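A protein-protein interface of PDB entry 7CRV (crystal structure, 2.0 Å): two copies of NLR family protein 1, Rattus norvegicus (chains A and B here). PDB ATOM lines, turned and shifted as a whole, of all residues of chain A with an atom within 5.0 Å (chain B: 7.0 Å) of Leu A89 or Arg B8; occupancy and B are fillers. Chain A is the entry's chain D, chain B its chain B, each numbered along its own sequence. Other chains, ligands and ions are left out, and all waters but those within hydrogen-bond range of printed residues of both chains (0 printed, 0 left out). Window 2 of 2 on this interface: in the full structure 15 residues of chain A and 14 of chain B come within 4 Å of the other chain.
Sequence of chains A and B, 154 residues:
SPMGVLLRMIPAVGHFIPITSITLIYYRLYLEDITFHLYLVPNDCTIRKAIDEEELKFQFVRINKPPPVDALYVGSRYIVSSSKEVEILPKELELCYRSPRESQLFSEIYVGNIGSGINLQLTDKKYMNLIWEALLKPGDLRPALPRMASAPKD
Hydrophobic or aromatic side chains of chain A that line the printed part of chain B: Leu A89 and Pro A90. Along chain A the printed residues that touch a printed residue of chain B span positions 88 to 91. Of the 9 printed residues of chain B, 5 touch a printed residue of chain A. Among the printed residues, 8 pairs touch across the chains. Among the printed residues, no Asp or Glu carboxylate lies within 4 Å of a Lys or Arg side-chain nitrogen of the other chain.
O of Ile A88 touches CB of Pro B11 (3.3 Å). Leu A89 touches Arg B8. Leu A89 touches Met B9. Leu A89 touches Ile B10 (CD1 to C, 3.7 Å). Leu A89 touches Pro B11. Pro A90 touches Met B9. CA of Gly B14 touches CB of Pro A90 (3.8 Å). Pro B11 touches Lys A91 (O to CG, 3.3 Å).
O of Leu A89 lies within hydrogen-bond range of N of Glu A108, at 2.8 Å. The side-chain hydroxyl (OG) of Ser A107 lies within hydrogen-bond range of the backbone carbonyl oxygen (O) of Pro A90 (2.9 Å).
Of chain B, only Arg B8, Met B9, Ile B10 and Pro B11 come within 4 Å of Leu A89. Printed residues of chain B within 4 Å of Lys A91: Pro B11. Of the printed residues of chain B, Pro A90 touches Met B9 (3.9 Å) and Gly B14 (3.8 Å). Printed residues of chain B within 4 Å of Ile A88: Pro B11 (3.3 Å). Printed residues of chain A within 4 Å of Met B9: Leu A89 and Pro A90. Of the printed residues of chain A, Pro B11 touches Ile A88 (3.3 Å), Leu A89 (3.5 Å) and Lys A91 (3.3 Å). Ser A107 touches none of the printed residues of chain B. The nearest printed residue of chain A that does not touch Pro B11 is Pro A90 (4.5 Å).
No position is printed for both chains.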
ATOM      1  N   GLU A  87      20.423 -20.142 -14.938  1.00  0.00           N
ATOM      2  CA  GLU A  87      20.906 -21.115 -13.961  1.00  0.00           C
ATOM      3  C   GLU A  87      21.217 -22.440 -14.657  1.00  0.00           C
ATOM      4  O   GLU A  87      20.365 -22.973 -15.382  1.00  0.00           O
ATOM      5  CB  GLU A  87      19.865 -21.333 -12.865  1.00  0.00           C
ATOM      6  CG  GLU A  87      19.202 -20.042 -12.404  1.00  0.00           C
ATOM      7  CD  GLU A  87      18.158 -20.281 -11.311  1.00  0.00           C
ATOM      8  OE1 GLU A  87      18.191 -21.374 -10.678  1.00  0.00           O
ATOM      9  OE2 GLU A  87      17.299 -19.382 -11.099  1.00  0.00           O
ATOM     10  N   ILE A  88      22.421 -22.978 -14.430  1.00  0.00           N
ATOM     11  CA  ILE A  88      22.861 -24.187 -15.127  1.00  0.00           C
ATOM     12  C   ILE A  88      23.285 -25.242 -14.111  1.00  0.00           C
ATOM     13  O   ILE A  88      24.177 -24.993 -13.295  1.00  0.00           O
ATOM     14  CB  ILE A  88      24.003 -23.889 -16.111  1.00  0.00           C
ATOM     15  CG1 ILE A  88      23.556 -22.843 -17.151  1.00  0.00           C
ATOM     16  CG2 ILE A  88      24.452 -25.188 -16.795  1.00  0.00           C
ATOM     17  CD1 ILE A  88      24.668 -22.213 -17.933  1.00  0.00           C
ATOM     18  N   LEU A  89      22.671 -26.437 -14.186  1.00  0.00           N
ATOM     19  CA  LEU A  89      22.932 -27.518 -13.235  1.00  0.00           C
ATOM     20  C   LEU A  89      22.981 -28.884 -13.918  1.00  0.00           C
ATOM     21  O   LEU A  89      21.952 -29.358 -14.409  1.00  0.00           O
ATOM     22  CB  LEU A  89      21.853 -27.534 -12.138  1.00  0.00           C
ATOM     23  CG  LEU A  89      22.053 -28.684 -11.144  1.00  0.00           C
ATOM     24  CD1 LEU A  89      23.319 -28.445 -10.305  1.00  0.00           C
ATOM     25  CD2 LEU A  89      20.837 -28.892 -10.240  1.00  0.00           C
ATOM     26  N   PRO A  90      24.155 -29.551 -14.003  1.00  0.00           N
ATOM     27  CA  PRO A  90      25.514 -29.091 -13.674  1.00  0.00           C
ATOM     28  C   PRO A  90      26.153 -28.283 -14.805  1.00  0.00           C
ATOM     29  O   PRO A  90      25.630 -28.316 -15.926  1.00  0.00           O
ATOM     30  CB  PRO A  90      26.281 -30.396 -13.451  1.00  0.00           C
ATOM     31  CG  PRO A  90      25.564 -31.406 -14.293  1.00  0.00           C
ATOM     32  CD  PRO A  90      24.124 -30.973 -14.392  1.00  0.00           C
ATOM     33  N   LYS A  91      27.250 -27.573 -14.503  1.00  0.00           N
ATOM     34  CA  LYS A  91      27.992 -26.815 -15.513  1.00  0.00           C
ATOM     35  C   LYS A  91      28.880 -27.709 -16.368  1.00  0.00           C
ATOM     36  O   LYS A  91      29.214 -27.321 -17.492  1.00  0.00           O
ATOM     37  CB  LYS A  91      28.889 -25.749 -14.873  1.00  0.00           C
ATOM     38  CG  LYS A  91      28.202 -24.719 -14.000  1.00  0.00           C
ATOM     39  CD  LYS A  91      27.811 -23.456 -14.782  1.00  0.00           C
ATOM     40  CE  LYS A  91      27.708 -22.234 -13.862  1.00  0.00           C
ATOM     41  NZ  LYS A  91      26.866 -21.142 -14.449  1.00  0.00           N
ATOM     42  N   PHE A 106      22.401 -34.989 -18.469  1.00  0.00           N
ATOM     43  CA  PHE A 106      22.138 -33.763 -19.190  1.00  0.00           C
ATOM     44  C   PHE A 106      22.404 -32.602 -18.255  1.00  0.00           C
ATOM     45  O   PHE A 106      22.484 -32.766 -17.036  1.00  0.00           O
ATOM     46  CB  PHE A 106      20.703 -33.719 -19.736  1.00  0.00           C
ATOM     47  CG  PHE A 106      19.610 -33.687 -18.674  1.00  0.00           C
ATOM     48  CD1 PHE A 106      19.199 -32.487 -18.112  1.00  0.00           C
ATOM     49  CD2 PHE A 106      18.939 -34.845 -18.310  1.00  0.00           C
ATOM     50  CE1 PHE A 106      18.171 -32.439 -17.171  1.00  0.00           C
ATOM     51  CE2 PHE A 106      17.907 -34.804 -17.379  1.00  0.00           C
ATOM     52  CZ  PHE A 106      17.517 -33.606 -16.812  1.00  0.00           C
ATOM     53  N   SER A 107      22.536 -31.424 -18.841  1.00  0.00           N
ATOM     54  CA  SER A 107      22.627 -30.188 -18.091  1.00  0.00           C
ATOM     55  C   SER A 107      21.281 -29.460 -18.147  1.00  0.00           C
ATOM     56  O   SER A 107      20.690 -29.317 -19.222  1.00  0.00           O
ATOM     57  CB  SER A 107      23.760 -29.337 -18.656  1.00  0.00           C
ATOM     58  OG  SER A 107      23.771 -28.038 -18.115  1.00  0.00           O
ATOM     59  N   GLU A 108      20.795 -29.016 -16.990  1.00  0.00           N
ATOM     60  CA  GLU A 108      19.514 -28.333 -16.891  1.00  0.00           C
ATOM     61  C   GLU A 108      19.735 -26.830 -16.887  1.00  0.00           C
ATOM     62  O   GLU A 108      20.434 -26.298 -16.020  1.00  0.00           O
ATOM     63  CB  GLU A 108      18.774 -28.756 -15.626  1.00  0.00           C
ATOM     64  CG  GLU A 108      17.372 -28.193 -15.520  1.00  0.00           C
ATOM     65  CD  GLU A 108      16.781 -28.471 -14.158  1.00  0.00           C
ATOM     66  OE1 GLU A 108      15.834 -29.290 -14.087  1.00  0.00           O
ATOM     67  OE2 GLU A 108      17.289 -27.892 -13.165  1.00  0.00           O
ATOM     68  N   LEU B   6      20.489 -39.514  -0.601  1.00  0.00           N
ATOM     69  CA  LEU B   6      20.700 -38.644  -1.752  1.00  0.00           C
ATOM     70  C   LEU B   6      21.393 -37.363  -1.302  1.00  0.00           C
ATOM     71  O   LEU B   6      21.219 -36.927  -0.161  1.00  0.00           O
ATOM     72  CB  LEU B   6      19.367 -38.275  -2.423  1.00  0.00           C
ATOM     73  CG  LEU B   6      18.645 -39.403  -3.158  1.00  0.00           C
ATOM     74  CD1 LEU B   6      17.289 -38.913  -3.665  1.00  0.00           C
ATOM     75  CD2 LEU B   6      19.474 -39.940  -4.317  1.00  0.00           C
ATOM     76  N   LEU B   7      22.172 -36.751  -2.198  1.00  0.00           N
ATOM     77  CA  LEU B   7      22.818 -35.471  -1.922  1.00  0.00           C
ATOM     78  C   LEU B   7      22.403 -34.450  -2.977  1.00  0.00           C
ATOM     79  O   LEU B   7      22.517 -34.723  -4.179  1.00  0.00           O
ATOM     80  CB  LEU B   7      24.338 -35.608  -1.902  1.00  0.00           C
ATOM     81  CG  LEU B   7      25.120 -34.310  -1.659  1.00  0.00           C
ATOM     82  CD1 LEU B   7      24.943 -33.820  -0.200  1.00  0.00           C
ATOM     83  CD2 LEU B   7      26.588 -34.497  -2.001  1.00  0.00           C
ATOM     84  N   ARG B   8      21.908 -33.284  -2.535  1.00  0.00           N
ATOM     85  CA  ARG B   8      21.495 -32.242  -3.478  1.00  0.00           C
ATOM     86  C   ARG B   8      22.727 -31.618  -4.122  1.00  0.00           C
ATOM     87  O   ARG B   8      23.645 -31.188  -3.423  1.00  0.00           O
ATOM     88  CB  ARG B   8      20.645 -31.169  -2.775  1.00  0.00           C
ATOM     89  CG  ARG B   8      20.207 -29.944  -3.625  1.00  0.00           C
ATOM     90  CD  ARG B   8      19.244 -30.346  -4.731  1.00  0.00           C
ATOM     91  NE  ARG B   8      18.376 -29.279  -5.272  1.00  0.00           N
ATOM     92  CZ  ARG B   8      18.734 -28.328  -6.152  1.00  0.00           C
ATOM     93  NH1 ARG B   8      19.979 -28.258  -6.635  1.00  0.00           N
ATOM     94  NH2 ARG B   8      17.822 -27.447  -6.583  1.00  0.00           N
ATOM     95  N   MET B   9      22.746 -31.591  -5.454  1.00  0.00           N
ATOM     96  CA  MET B   9      23.811 -30.962  -6.219  1.00  0.00           C
ATOM     97  C   MET B   9      23.732 -29.434  -6.187  1.00  0.00           C
ATOM     98  O   MET B   9      22.649 -28.837  -6.129  1.00  0.00           O
ATOM     99  CB  MET B   9      23.738 -31.400  -7.673  1.00  0.00           C
ATOM    100  CG  MET B   9      24.691 -32.456  -8.009  1.00  0.00           C
ATOM    101  SD  MET B   9      24.263 -33.263  -9.540  1.00  0.00           S
ATOM    102  CE  MET B   9      23.964 -31.868 -10.647  1.00  0.00           C
ATOM    103  N   ILE B  10      24.900 -28.810  -6.324  1.00  0.00           N
ATOM    104  CA  ILE B  10      25.051 -27.356  -6.410  1.00  0.00           C
ATOM    105  C   ILE B  10      25.602 -27.013  -7.791  1.00  0.00           C
ATOM    106  O   ILE B  10      26.522 -27.697  -8.267  1.00  0.00           O
ATOM    107  CB  ILE B  10      25.967 -26.830  -5.293  1.00  0.00           C
ATOM    108  CG1 ILE B  10      25.298 -27.017  -3.931  1.00  0.00           C
ATOM    109  CG2 ILE B  10      26.380 -25.385  -5.557  1.00  0.00           C
ATOM    110  CD1 ILE B  10      23.919 -26.393  -3.828  1.00  0.00           C
ATOM    111  N   PRO B  11      25.076 -25.981  -8.470  1.00  0.00           N
ATOM    112  CA  PRO B  11      25.529 -25.693  -9.848  1.00  0.00           C
ATOM    113  C   PRO B  11      27.036 -25.611 -10.003  1.00  0.00           C
ATOM    114  O   PRO B  11      27.585 -26.086 -11.008  1.00  0.00           O
ATOM    115  CB  PRO B  11      24.855 -24.350 -10.149  1.00  0.00           C
ATOM    116  CG  PRO B  11      23.573 -24.425  -9.397  1.00  0.00           C
ATOM    117  CD  PRO B  11      23.919 -25.147  -8.092  1.00  0.00           C
ATOM    118  N   ALA B  12      27.715 -25.058  -9.000  1.00  0.00           N
ATOM    119  CA  ALA B  12      29.165 -24.921  -9.046  1.00  0.00           C
ATOM    120  C   ALA B  12      29.882 -26.269  -9.078  1.00  0.00           C
ATOM    121  O   ALA B  12      30.981 -26.370  -9.630  1.00  0.00           O
ATOM    122  CB  ALA B  12      29.637 -24.124  -7.831  1.00  0.00           C
ATOM    123  N   VAL B  13      29.282 -27.313  -8.502  1.00  0.00           N
ATOM    124  CA  VAL B  13      29.990 -28.534  -8.141  1.00  0.00           C
ATOM    125  C   VAL B  13      29.586 -29.700  -9.039  1.00  0.00           C
ATOM    126  O   VAL B  13      30.441 -30.439  -9.539  1.00  0.00           O
ATOM    127  CB  VAL B  13      29.737 -28.876  -6.654  1.00  0.00           C
ATOM    128  CG1 VAL B  13      30.608 -30.060  -6.218  1.00  0.00           C
ATOM    129  CG2 VAL B  13      29.812 -27.640  -5.757  1.00  0.00           C
ATOM    130  N   GLY B  14      28.281 -29.907  -9.219  1.00  0.00           N
ATOM    131  CA  GLY B  14      27.867 -31.034 -10.047  1.00  0.00           C
ATOM    132  C   GLY B  14      28.176 -32.394  -9.421  1.00  0.00           C
ATOM    133  O   GLY B  14      28.227 -32.550  -8.204  1.00  0.00           O
